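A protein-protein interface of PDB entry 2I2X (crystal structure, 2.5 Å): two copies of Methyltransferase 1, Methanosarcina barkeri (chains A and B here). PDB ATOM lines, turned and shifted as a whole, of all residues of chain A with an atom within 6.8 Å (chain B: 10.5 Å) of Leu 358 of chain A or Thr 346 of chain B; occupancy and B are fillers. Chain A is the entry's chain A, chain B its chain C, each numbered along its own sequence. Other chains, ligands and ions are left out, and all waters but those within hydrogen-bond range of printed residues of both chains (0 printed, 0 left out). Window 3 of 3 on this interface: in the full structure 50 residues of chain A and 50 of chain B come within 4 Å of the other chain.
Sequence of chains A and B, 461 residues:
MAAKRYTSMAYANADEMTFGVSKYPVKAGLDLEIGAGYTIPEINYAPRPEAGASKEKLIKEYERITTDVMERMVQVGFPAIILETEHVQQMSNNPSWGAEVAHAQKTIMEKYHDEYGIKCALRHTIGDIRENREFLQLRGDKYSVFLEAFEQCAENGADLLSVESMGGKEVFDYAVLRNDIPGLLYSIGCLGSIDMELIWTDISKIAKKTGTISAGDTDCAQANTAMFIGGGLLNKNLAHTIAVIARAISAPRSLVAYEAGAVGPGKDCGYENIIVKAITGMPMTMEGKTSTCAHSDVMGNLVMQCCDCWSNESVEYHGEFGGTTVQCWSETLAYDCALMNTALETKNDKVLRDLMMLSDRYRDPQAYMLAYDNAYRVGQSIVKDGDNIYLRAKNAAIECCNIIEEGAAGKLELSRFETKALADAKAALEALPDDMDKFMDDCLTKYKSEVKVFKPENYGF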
ATOM      1  N   LEU A 302     -16.295  24.731   7.903  1.00  0.00           N
ATOM      2  CA  LEU A 302     -15.425  23.608   8.119  1.00  0.00           C
ATOM      3  C   LEU A 302     -15.288  23.239   9.606  1.00  0.00           C
ATOM      4  O   LEU A 302     -15.248  22.046   9.933  1.00  0.00           O
ATOM      5  CB  LEU A 302     -14.069  23.877   7.497  1.00  0.00           C
ATOM      6  CG  LEU A 302     -12.944  22.853   7.704  1.00  0.00           C
ATOM      7  CD1 LEU A 302     -12.005  22.905   6.552  1.00  0.00           C
ATOM      8  CD2 LEU A 302     -12.221  23.075   9.024  1.00  0.00           C
ATOM      9  N   GLN A 305     -17.351  20.487  11.423  1.00  0.00           N
ATOM     10  CA  GLN A 305     -17.203  19.136  10.893  1.00  0.00           C
ATOM     11  C   GLN A 305     -17.206  18.077  12.002  1.00  0.00           C
ATOM     12  O   GLN A 305     -17.705  16.975  11.808  1.00  0.00           O
ATOM     13  CB  GLN A 305     -15.911  19.060  10.069  1.00  0.00           C
ATOM     14  CG  GLN A 305     -14.637  19.170  10.936  1.00  0.00           C
ATOM     15  CD  GLN A 305     -13.370  19.492  10.165  1.00  0.00           C
ATOM     16  OE1 GLN A 305     -13.205  19.135   9.001  1.00  0.00           O
ATOM     17  NE2 GLN A 305     -12.444  20.149  10.842  1.00  0.00           N
ATOM     18  N   VAL A 351     -21.852  12.608   5.787  1.00  0.00           N
ATOM     19  CA  VAL A 351     -21.903  13.345   4.532  1.00  0.00           C
ATOM     20  C   VAL A 351     -21.975  14.845   4.825  1.00  0.00           C
ATOM     21  O   VAL A 351     -21.386  15.656   4.115  1.00  0.00           O
ATOM     22  CB  VAL A 351     -23.097  12.906   3.609  1.00  0.00           C
ATOM     23  CG1 VAL A 351     -24.410  13.147   4.287  1.00  0.00           C
ATOM     24  CG2 VAL A 351     -23.100  13.678   2.268  1.00  0.00           C
ATOM     25  N   LEU A 352     -22.696  15.208   5.879  1.00  0.00           N
ATOM     26  CA  LEU A 352     -22.840  16.610   6.228  1.00  0.00           C
ATOM     27  C   LEU A 352     -21.507  17.108   6.739  1.00  0.00           C
ATOM     28  O   LEU A 352     -21.029  18.165   6.301  1.00  0.00           O
ATOM     29  CB  LEU A 352     -23.990  16.840   7.231  1.00  0.00           C
ATOM     30  CG  LEU A 352     -24.193  18.296   7.687  1.00  0.00           C
ATOM     31  CD1 LEU A 352     -24.446  19.212   6.486  1.00  0.00           C
ATOM     32  CD2 LEU A 352     -25.283  18.411   8.733  1.00  0.00           C
ATOM     33  N   ARG A 353     -20.889  16.340   7.638  1.00  0.00           N
ATOM     34  CA  ARG A 353     -19.483  16.560   7.991  1.00  0.00           C
ATOM     35  C   ARG A 353     -18.593  16.808   6.749  1.00  0.00           C
ATOM     36  O   ARG A 353     -17.946  17.847   6.646  1.00  0.00           O
ATOM     37  CB  ARG A 353     -18.987  15.429   8.872  1.00  0.00           C
ATOM     38  CG  ARG A 353     -17.439  15.296   9.076  1.00  0.00           C
ATOM     39  CD  ARG A 353     -16.986  14.181   8.157  1.00  0.00           C
ATOM     40  NE  ARG A 353     -16.630  12.996   8.885  1.00  0.00           N
ATOM     41  CZ  ARG A 353     -16.516  11.774   8.381  1.00  0.00           C
ATOM     42  NH1 ARG A 353     -16.772  11.520   7.107  1.00  0.00           N
ATOM     43  NH2 ARG A 353     -16.112  10.802   9.209  1.00  0.00           N
ATOM     44  N   ASP A 354     -18.627  15.933   5.755  1.00  0.00           N
ATOM     45  CA  ASP A 354     -17.842  16.209   4.547  1.00  0.00           C
ATOM     46  C   ASP A 354     -18.206  17.506   3.832  1.00  0.00           C
ATOM     47  O   ASP A 354     -17.320  18.209   3.336  1.00  0.00           O
ATOM     48  CB  ASP A 354     -17.848  15.025   3.593  1.00  0.00           C
ATOM     49  CG  ASP A 354     -17.112  13.824   4.166  1.00  0.00           C
ATOM     50  OD1 ASP A 354     -16.384  13.940   5.198  1.00  0.00           O
ATOM     51  OD2 ASP A 354     -17.250  12.744   3.578  1.00  0.00           O
ATOM     52  N   LEU A 355     -19.502  17.831   3.798  1.00  0.00           N
ATOM     53  CA  LEU A 355     -19.983  19.009   3.093  1.00  0.00           C
ATOM     54  C   LEU A 355     -19.422  20.265   3.803  1.00  0.00           C
ATOM     55  O   LEU A 355     -18.854  21.160   3.169  1.00  0.00           O
ATOM     56  CB  LEU A 355     -21.514  19.008   3.059  1.00  0.00           C
ATOM     57  CG  LEU A 355     -22.412  18.753   1.832  1.00  0.00           C
ATOM     58  CD1 LEU A 355     -21.749  18.153   0.627  1.00  0.00           C
ATOM     59  CD2 LEU A 355     -23.599  17.921   2.228  1.00  0.00           C
ATOM     60  N   MET A 356     -19.527  20.287   5.126  1.00  0.00           N
ATOM     61  CA  MET A 356     -19.003  21.402   5.922  1.00  0.00           C
ATOM     62  C   MET A 356     -17.515  21.544   5.682  1.00  0.00           C
ATOM     63  O   MET A 356     -17.026  22.648   5.490  1.00  0.00           O
ATOM     64  CB  MET A 356     -19.282  21.205   7.421  1.00  0.00           C
ATOM     65  CG  MET A 356     -20.723  20.976   7.701  1.00  0.00           C
ATOM     66  SD  MET A 356     -21.130  20.581   9.395  1.00  0.00           S
ATOM     67  CE  MET A 356     -19.959  19.338   9.711  1.00  0.00           C
ATOM     68  N   MET A 357     -16.811  20.418   5.644  1.00  0.00           N
ATOM     69  CA  MET A 357     -15.375  20.436   5.483  1.00  0.00           C
ATOM     70  C   MET A 357     -15.060  20.972   4.092  1.00  0.00           C
ATOM     71  O   MET A 357     -14.295  21.931   3.954  1.00  0.00           O
ATOM     72  CB  MET A 357     -14.781  19.032   5.735  1.00  0.00           C
ATOM     73  CG  MET A 357     -13.285  18.890   5.480  1.00  0.00           C
ATOM     74  SD  MET A 357     -12.787  18.854   3.726  1.00  0.00           S
ATOM     75  CE  MET A 357     -13.569  17.322   3.162  1.00  0.00           C
ATOM     76  N   LEU A 358     -15.636  20.355   3.071  1.00  0.00           N
ATOM     77  CA  LEU A 358     -15.316  20.705   1.664  1.00  0.00           C
ATOM     78  C   LEU A 358     -15.601  22.185   1.312  1.00  0.00           C
ATOM     79  O   LEU A 358     -14.871  22.813   0.504  1.00  0.00           O
ATOM     80  CB  LEU A 358     -16.022  19.756   0.668  1.00  0.00           C
ATOM     81  CG  LEU A 358     -15.691  19.966  -0.812  1.00  0.00           C
ATOM     82  CD1 LEU A 358     -14.173  19.869  -1.062  1.00  0.00           C
ATOM     83  CD2 LEU A 358     -16.451  18.974  -1.711  1.00  0.00           C
ATOM     84  N   SER A 359     -16.661  22.716   1.916  1.00  0.00           N
ATOM     85  CA  SER A 359     -17.019  24.144   1.850  1.00  0.00           C
ATOM     86  C   SER A 359     -15.807  25.079   1.937  1.00  0.00           C
ATOM     87  O   SER A 359     -15.664  26.043   1.165  1.00  0.00           O
ATOM     88  CB  SER A 359     -17.977  24.459   3.004  1.00  0.00           C
ATOM     89  OG  SER A 359     -18.125  25.864   3.194  1.00  0.00           O
ATOM     90  N   ASP A 360     -14.934  24.798   2.885  1.00  0.00           N
ATOM     91  CA  ASP A 360     -13.873  25.724   3.211  1.00  0.00           C
ATOM     92  C   ASP A 360     -12.485  25.166   2.955  1.00  0.00           C
ATOM     93  O   ASP A 360     -11.531  25.925   3.022  1.00  0.00           O
ATOM     94  CB  ASP A 360     -13.991  26.147   4.677  1.00  0.00           C
ATOM     95  CG  ASP A 360     -15.277  26.906   4.965  1.00  0.00           C
ATOM     96  OD1 ASP A 360     -15.788  27.546   4.039  1.00  0.00           O
ATOM     97  OD2 ASP A 360     -15.768  26.888   6.119  1.00  0.00           O
ATOM     98  N   ARG A 361     -12.366  23.865   2.654  1.00  0.00           N
ATOM     99  CA  ARG A 361     -11.062  23.255   2.427  1.00  0.00           C
ATOM    100  C   ARG A 361     -10.134  24.110   1.538  1.00  0.00           C
ATOM    101  O   ARG A 361      -8.905  24.133   1.782  1.00  0.00           O
ATOM    102  CB  ARG A 361     -11.154  21.784   1.890  1.00  0.00           C
ATOM    103  CG  ARG A 361      -9.795  21.260   1.299  1.00  0.00           C
ATOM    104  CD  ARG A 361      -9.785  19.807   0.745  1.00  0.00           C
ATOM    105  NE  ARG A 361      -9.925  18.978   1.901  1.00  0.00           N
ATOM    106  CZ  ARG A 361      -9.096  18.048   2.343  1.00  0.00           C
ATOM    107  NH1 ARG A 361      -8.004  17.694   1.683  1.00  0.00           N
ATOM    108  NH2 ARG A 361      -9.439  17.445   3.475  1.00  0.00           N
ATOM    109  N   TYR A 362     -10.697  24.793   0.529  1.00  0.00           N
ATOM    110  CA  TYR A 362      -9.848  25.509  -0.447  1.00  0.00           C
ATOM    111  C   TYR A 362      -9.823  27.028  -0.256  1.00  0.00           C
ATOM    112  O   TYR A 362      -9.132  27.762  -0.997  1.00  0.00           O
ATOM    113  CB  TYR A 362     -10.186  25.116  -1.905  1.00  0.00           C
ATOM    114  CG  TYR A 362      -9.940  23.635  -2.181  1.00  0.00           C
ATOM    115  CD1 TYR A 362      -8.634  23.115  -2.257  1.00  0.00           C
ATOM    116  CD2 TYR A 362     -11.012  22.742  -2.319  1.00  0.00           C
ATOM    117  CE1 TYR A 362      -8.411  21.747  -2.484  1.00  0.00           C
ATOM    118  CE2 TYR A 362     -10.802  21.381  -2.536  1.00  0.00           C
ATOM    119  CZ  TYR A 362      -9.503  20.889  -2.636  1.00  0.00           C
ATOM    120  OH  TYR A 362      -9.312  19.541  -2.851  1.00  0.00           O
ATOM    121  N   ARG A 363     -10.555  27.487   0.753  1.00  0.00           N
ATOM    122  CA  ARG A 363     -10.630  28.893   1.019  1.00  0.00           C
ATOM    123  C   ARG A 363      -9.286  29.518   1.396  1.00  0.00           C
ATOM    124  O   ARG A 363      -9.049  30.667   1.029  1.00  0.00           O
ATOM    125  CB  ARG A 363     -11.661  29.179   2.105  1.00  0.00           C
ATOM    126  CG  ARG A 363     -12.387  30.548   1.978  1.00  0.00           C
ATOM    127  CD  ARG A 363     -13.525  30.614   3.011  1.00  0.00           C
ATOM    128  NE  ARG A 363     -14.615  29.788   2.523  1.00  0.00           N
ATOM    129  CZ  ARG A 363     -15.504  30.177   1.604  1.00  0.00           C
ATOM    130  NH1 ARG A 363     -15.451  31.395   1.048  1.00  0.00           N
ATOM    131  NH2 ARG A 363     -16.414  29.323   1.206  1.00  0.00           N
ATOM    132  N   ALA A 371      -8.967  20.892   8.128  1.00  0.00           N
ATOM    133  CA  ALA A 371      -9.864  19.839   7.610  1.00  0.00           C
ATOM    134  C   ALA A 371      -9.589  18.489   8.313  1.00  0.00           C
ATOM    135  O   ALA A 371      -8.449  18.085   8.451  1.00  0.00           O
ATOM    136  CB  ALA A 371      -9.715  19.714   6.116  1.00  0.00           C
ATOM    137  N   PHE B  19     -32.733  23.647  -3.477  1.00  0.00           N
ATOM    138  CA  PHE B  19     -32.272  25.016  -3.301  1.00  0.00           C
ATOM    139  C   PHE B  19     -31.312  25.449  -4.443  1.00  0.00           C
ATOM    140  O   PHE B  19     -30.570  24.615  -4.993  1.00  0.00           O
ATOM    141  CB  PHE B  19     -31.648  25.207  -1.905  1.00  0.00           C
ATOM    142  CG  PHE B  19     -30.632  24.151  -1.510  1.00  0.00           C
ATOM    143  CD1 PHE B  19     -30.904  23.264  -0.497  1.00  0.00           C
ATOM    144  CD2 PHE B  19     -29.387  24.073  -2.129  1.00  0.00           C
ATOM    145  CE1 PHE B  19     -29.936  22.277  -0.087  1.00  0.00           C
ATOM    146  CE2 PHE B  19     -28.446  23.118  -1.745  1.00  0.00           C
ATOM    147  CZ  PHE B  19     -28.718  22.215  -0.729  1.00  0.00           C
ATOM    148  N   GLY B  37     -28.287  27.407 -10.207  1.00  0.00           N
ATOM    149  CA  GLY B  37     -27.416  26.373  -9.684  1.00  0.00           C
ATOM    150  C   GLY B  37     -26.475  26.876  -8.601  1.00  0.00           C
ATOM    151  O   GLY B  37     -25.448  26.258  -8.346  1.00  0.00           O
ATOM    152  N   TYR B 335     -21.765  32.116   4.151  1.00  0.00           N
ATOM    153  CA  TYR B 335     -21.291  30.794   4.513  1.00  0.00           C
ATOM    154  C   TYR B 335     -22.439  29.786   4.431  1.00  0.00           C
ATOM    155  O   TYR B 335     -22.234  28.659   3.957  1.00  0.00           O
ATOM    156  CB  TYR B 335     -20.659  30.783   5.920  1.00  0.00           C
ATOM    157  CG  TYR B 335     -19.168  31.026   6.010  1.00  0.00           C
ATOM    158  CD1 TYR B 335     -18.264  30.188   5.356  1.00  0.00           C
ATOM    159  CD2 TYR B 335     -18.664  32.072   6.784  1.00  0.00           C
ATOM    160  CE1 TYR B 335     -16.894  30.380   5.455  1.00  0.00           C
ATOM    161  CE2 TYR B 335     -17.260  32.311   6.885  1.00  0.00           C
ATOM    162  CZ  TYR B 335     -16.394  31.450   6.219  1.00  0.00           C
ATOM    163  OH  TYR B 335     -15.045  31.630   6.316  1.00  0.00           O
ATOM    164  N   CYS B 337     -24.851  29.871   2.402  1.00  0.00           N
ATOM    165  CA  CYS B 337     -24.954  29.634   0.991  1.00  0.00           C
ATOM    166  C   CYS B 337     -23.783  28.788   0.486  1.00  0.00           C
ATOM    167  O   CYS B 337     -23.986  27.950  -0.397  1.00  0.00           O
ATOM    168  CB  CYS B 337     -25.028  30.947   0.215  1.00  0.00           C
ATOM    169  SG  CYS B 337     -26.568  31.883   0.409  1.00  0.00           S
ATOM    170  N   ALA B 338     -22.577  28.966   1.044  1.00  0.00           N
ATOM    171  CA  ALA B 338     -21.455  28.076   0.652  1.00  0.00           C
ATOM    172  C   ALA B 338     -21.705  26.585   0.938  1.00  0.00           C
ATOM    173  O   ALA B 338     -21.337  25.714   0.141  1.00  0.00           O
ATOM    174  CB  ALA B 338     -20.136  28.521   1.263  1.00  0.00           C
ATOM    175  N   LEU B 339     -22.312  26.296   2.092  1.00  0.00           N
ATOM    176  CA  LEU B 339     -22.660  24.917   2.476  1.00  0.00           C
ATOM    177  C   LEU B 339     -23.598  24.364   1.404  1.00  0.00           C
ATOM    178  O   LEU B 339     -23.386  23.276   0.869  1.00  0.00           O
ATOM    179  CB  LEU B 339     -23.342  24.894   3.838  1.00  0.00           C
ATOM    180  CG  LEU B 339     -23.613  23.504   4.372  1.00  0.00           C
ATOM    181  CD1 LEU B 339     -22.295  22.730   4.633  1.00  0.00           C
ATOM    182  CD2 LEU B 339     -24.481  23.546   5.633  1.00  0.00           C
ATOM    183  N   MET B 340     -24.613  25.162   1.058  1.00  0.00           N
ATOM    184  CA  MET B 340     -25.622  24.731   0.105  1.00  0.00           C
ATOM    185  C   MET B 340     -24.993  24.537  -1.277  1.00  0.00           C
ATOM    186  O   MET B 340     -25.267  23.551  -1.970  1.00  0.00           O
ATOM    187  CB  MET B 340     -26.787  25.733   0.073  1.00  0.00           C
ATOM    188  CG  MET B 340     -27.826  25.573   1.208  1.00  0.00           C
ATOM    189  SD  MET B 340     -29.250  26.697   1.032  1.00  0.00           S
ATOM    190  CE  MET B 340     -28.637  28.272   1.668  1.00  0.00           C
ATOM    191  N   ASN B 341     -24.130  25.464  -1.674  1.00  0.00           N
ATOM    192  CA  ASN B 341     -23.470  25.337  -2.962  1.00  0.00           C
ATOM    193  C   ASN B 341     -22.531  24.154  -3.062  1.00  0.00           C
ATOM    194  O   ASN B 341     -22.455  23.533  -4.153  1.00  0.00           O
ATOM    195  CB  ASN B 341     -22.790  26.618  -3.351  1.00  0.00           C
ATOM    196  CG  ASN B 341     -23.773  27.774  -3.453  1.00  0.00           C
ATOM    197  OD1 ASN B 341     -25.004  27.569  -3.536  1.00  0.00           O
ATOM    198  ND2 ASN B 341     -23.240  28.997  -3.439  1.00  0.00           N
ATOM    199  N   THR B 342     -21.859  23.814  -1.941  1.00  0.00           N
ATOM    200  CA  THR B 342     -21.041  22.613  -1.874  1.00  0.00           C
ATOM    201  C   THR B 342     -21.943  21.394  -2.048  1.00  0.00           C
ATOM    202  O   THR B 342     -21.615  20.477  -2.799  1.00  0.00           O
ATOM    203  CB  THR B 342     -20.210  22.529  -0.538  1.00  0.00           C
ATOM    204  OG1 THR B 342     -19.400  23.705  -0.403  1.00  0.00           O
ATOM    205  CG2 THR B 342     -19.320  21.339  -0.520  1.00  0.00           C
ATOM    206  N   ALA B 343     -23.105  21.387  -1.417  1.00  0.00           N
ATOM    207  CA  ALA B 343     -24.040  20.278  -1.641  1.00  0.00           C
ATOM    208  C   ALA B 343     -24.482  20.171  -3.108  1.00  0.00           C
ATOM    209  O   ALA B 343     -24.523  19.096  -3.658  1.00  0.00           O
ATOM    210  CB  ALA B 343     -25.220  20.338  -0.704  1.00  0.00           C
ATOM    211  N   LEU B 344     -24.760  21.279  -3.757  1.00  0.00           N
ATOM    212  CA  LEU B 344     -25.137  21.229  -5.157  1.00  0.00           C
ATOM    213  C   LEU B 344     -24.037  20.648  -5.999  1.00  0.00           C
ATOM    214  O   LEU B 344     -24.283  19.746  -6.780  1.00  0.00           O
ATOM    215  CB  LEU B 344     -25.504  22.617  -5.685  1.00  0.00           C
ATOM    216  CG  LEU B 344     -26.881  23.074  -5.240  1.00  0.00           C
ATOM    217  CD1 LEU B 344     -26.942  24.595  -5.254  1.00  0.00           C
ATOM    218  CD2 LEU B 344     -28.022  22.443  -6.097  1.00  0.00           C
ATOM    219  N   GLU B 345     -22.826  21.180  -5.844  1.00  0.00           N
ATOM    220  CA  GLU B 345     -21.670  20.799  -6.692  1.00  0.00           C
ATOM    221  C   GLU B 345     -21.320  19.329  -6.567  1.00  0.00           C
ATOM    222  O   GLU B 345     -20.746  18.750  -7.492  1.00  0.00           O
ATOM    223  CB  GLU B 345     -20.431  21.655  -6.368  1.00  0.00           C
ATOM    224  CG  GLU B 345     -20.590  23.130  -6.732  1.00  0.00           C
ATOM    225  CD  GLU B 345     -21.013  23.362  -8.174  1.00  0.00           C
ATOM    226  OE1 GLU B 345     -20.522  22.649  -9.089  1.00  0.00           O
ATOM    227  OE2 GLU B 345     -21.828  24.283  -8.417  1.00  0.00           O
ATOM    228  N   THR B 346     -21.655  18.734  -5.420  1.00  0.00           N
ATOM    229  CA  THR B 346     -21.315  17.347  -5.169  1.00  0.00           C
ATOM    230  C   THR B 346     -22.525  16.448  -5.223  1.00  0.00           C
ATOM    231  O   THR B 346     -22.439  15.277  -4.839  1.00  0.00           O
ATOM    232  CB  THR B 346     -20.609  17.152  -3.795  1.00  0.00           C
ATOM    233  OG1 THR B 346     -21.507  17.493  -2.722  1.00  0.00           O
ATOM    234  CG2 THR B 346     -19.326  17.973  -3.715  1.00  0.00           C
ATOM    235  N   LYS B 347     -23.655  16.998  -5.687  1.00  0.00           N
ATOM    236  CA  LYS B 347     -24.924  16.263  -5.848  1.00  0.00           C
ATOM    237  C   LYS B 347     -25.399  15.681  -4.544  1.00  0.00           C
ATOM    238  O   LYS B 347     -25.890  14.561  -4.504  1.00  0.00           O
ATOM    239  CB  LYS B 347     -24.829  15.145  -6.905  1.00  0.00           C
ATOM    240  CG  LYS B 347     -25.042  15.614  -8.331  1.00  0.00           C
ATOM    241  CD  LYS B 347     -23.763  15.596  -9.159  1.00  0.00           C
ATOM    242  CE  LYS B 347     -23.596  16.891 -10.047  1.00  0.00           C
ATOM    243  NZ  LYS B 347     -24.849  17.361 -10.810  1.00  0.00           N
ATOM    244  N   ASN B 348     -25.255  16.440  -3.470  1.00  0.00           N
ATOM    245  CA  ASN B 348     -25.832  16.039  -2.201  1.00  0.00           C
ATOM    246  C   ASN B 348     -26.858  17.026  -1.732  1.00  0.00           C
ATOM    247  O   ASN B 348     -27.180  17.033  -0.549  1.00  0.00           O
ATOM    248  CB  ASN B 348     -24.754  15.921  -1.116  1.00  0.00           C
ATOM    249  CG  ASN B 348     -23.807  14.782  -1.351  1.00  0.00           C
ATOM    250  OD1 ASN B 348     -22.675  15.020  -1.724  1.00  0.00           O
ATOM    251  ND2 ASN B 348     -24.234  13.551  -1.079  1.00  0.00           N
ATOM    252  N   ASP B 349     -27.350  17.881  -2.631  1.00  0.00           N
ATOM    253  CA  ASP B 349     -28.349  18.888  -2.266  1.00  0.00           C
ATOM    254  C   ASP B 349     -29.614  18.279  -1.685  1.00  0.00           C
ATOM    255  O   ASP B 349     -30.106  18.766  -0.675  1.00  0.00           O
ATOM    256  CB  ASP B 349     -28.685  19.822  -3.433  1.00  0.00           C
ATOM    257  CG  ASP B 349     -29.004  19.074  -4.715  1.00  0.00           C
ATOM    258  OD1 ASP B 349     -28.098  18.397  -5.257  1.00  0.00           O
ATOM    259  OD2 ASP B 349     -30.165  19.164  -5.184  1.00  0.00           O
ATOM    260  N   LYS B 350     -30.125  17.211  -2.296  1.00  0.00           N
ATOM    261  CA  LYS B 350     -31.397  16.613  -1.862  1.00  0.00           C
ATOM    262  C   LYS B 350     -31.403  16.108  -0.436  1.00  0.00           C
ATOM    263  O   LYS B 350     -32.412  16.272   0.254  1.00  0.00           O
ATOM    264  CB  LYS B 350     -31.903  15.534  -2.832  1.00  0.00           C
ATOM    265  CG  LYS B 350     -32.410  16.179  -4.125  1.00  0.00           C
ATOM    266  CD  LYS B 350     -33.199  15.273  -5.085  1.00  0.00           C
ATOM    267  CE  LYS B 350     -33.609  16.119  -6.355  1.00  0.00           C
ATOM    268  NZ  LYS B 350     -34.663  15.473  -7.245  1.00  0.00           N
ATOM    269  N   VAL B 351     -30.296  15.523   0.030  1.00  0.00           N
ATOM    270  CA  VAL B 351     -30.264  15.024   1.414  1.00  0.00           C
ATOM    271  C   VAL B 351     -30.223  16.220   2.365  1.00  0.00           C
ATOM    272  O   VAL B 351     -30.931  16.253   3.386  1.00  0.00           O
ATOM    273  CB  VAL B 351     -29.087  14.011   1.708  1.00  0.00           C
ATOM    274  CG1 VAL B 351     -27.707  14.670   1.543  1.00  0.00           C
ATOM    275  CG2 VAL B 351     -29.188  13.426   3.133  1.00  0.00           C
ATOM    276  N   LEU B 352     -29.417  17.217   2.005  1.00  0.00           N
ATOM    277  CA  LEU B 352     -29.287  18.411   2.817  1.00  0.00           C
ATOM    278  C   LEU B 352     -30.629  19.126   2.854  1.00  0.00           C
ATOM    279  O   LEU B 352     -31.073  19.550   3.916  1.00  0.00           O
ATOM    280  CB  LEU B 352     -28.138  19.305   2.336  1.00  0.00           C
ATOM    281  CG  LEU B 352     -27.876  20.626   3.106  1.00  0.00           C
ATOM    282  CD1 LEU B 352     -27.690  20.459   4.652  1.00  0.00           C
ATOM    283  CD2 LEU B 352     -26.755  21.463   2.496  1.00  0.00           C
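Asn 348 of chain B touches Val 351 of chain A.
CD1 of Leu 352 of chain A touches CD1 of Leu 352 of chain B (3.9 Å).
Leu 355 of chain A touches Leu 339 of chain B.
Thr 342 of chain B touches Leu 355 of chain A (CG2 to O, 3.7 Å).
Thr 346 of chain B touches Leu 355 of chain A.
Met 356 of chain A touches Leu 339 of chain B.
CB of Leu 358 of chain A touches CG2 of Thr 342 of chain B, 3.8 Å away.
CD2 of Leu 358 of chain A touches CG2 of Thr 346 of chain B (3.6 Å).
Ser 359 of chain A touches Thr 342 of chain B.
OD1 of Asp 360 of chain A touches CE1 of Tyr 335 of chain B, 3.4 Å away.
The backbone NH (N) of Leu 302 of chain A sits at hydrogen-bond distance from the side-chain carboxylate (OD2) of Asp 360 of chain A (2.8 Å).
The backbone carbonyl oxygen (O) of Met 356 of chain A lies close to the backbone NH (N) of Leu 302 of chain A (3.3 Å).
The backbone NH (N) of Asn 348 of chain B sits at hydrogen-bond distance from the backbone carbonyl oxygen (O) of Ala 343 of chain B.
The guanidinium group (NH2) of Arg 363 of chain A sits at hydrogen-bond distance from the backbone carbonyl oxygen (O) of Ser 359 of chain A (3.4 Å).
The side-chain hydroxyl of Ser 359 of chain A is in hydrogen-bond range of the side-chain carboxylate of Asp 360 of chain A (3.0 Å).
The backbone carbonyl oxygen (O) of Ala 338 of chain B sits at hydrogen-bond distance from the side-chain hydroxyl (OG1) of Thr 342 of chain B (2.8 Å).
Of the 16 printed residues of chain A, 8 touch a printed residue of chain B.
Hydrophobic or aromatic side chains of chain A within 4 Å of the printed part of chain B: Val 351, Leu 352, Leu 355, Met 356 and Leu 358.
Of the 19 printed residues of chain B, 8 touch a printed residue of chain A.
Printed residues of chain B that touch a printed residue of chain A: Tyr 335, Ala 338, Leu 339, Thr 342, Ala 343, Thr 346, Asn 348 and Leu 352.
Among the printed residues, no Asp or Glu carboxylate lies within 4 Å of a Lys or Arg side-chain nitrogen of the other chain.
Leu 352 of chain A touches its own counterpart, Leu 352 of chain B.
2 positions are printed for both chains.
Of the 14 pairs that touch across the chains among the printed residues, 1 has its exchanged pair printed and touching as well.
Leu 358 of chain A touches just these residues of chain B: Thr 342 (3.8 Å) and Thr 346 (3.6 Å).
Of chain A, only Leu 355 (3.4 Å) and Leu 358 (3.6 Å) come within 4 Å of Thr 346 of chain B.
Ser 359 of chain A touches two residues of chain B.
Of the printed residues of chain A, Leu 352 of chain B touches Leu 352.
Of the printed residues of chain B, Arg 363 of chain A touches Tyr 335 and Ala 338.
Of the printed residues of chain B, Val 351 of chain A touches Asn 348.
Printed residues of chain A within 4 Å of Asn 348 of chain B: Val 351 (3.5 Å).
Of the printed residues of chain B, Leu 352 of chain A touches Leu 352 (3.9 Å).
Glu 345 of chain B touches none of the printed residues of chain A.
The nearest residue of chain B that does not touch Leu 358 of chain A is Glu 345 of chain B (6.7 Å).
The nearest residue of chain A that does not touch Thr 346 of chain B is Val 351 of chain A (6.5 Å).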
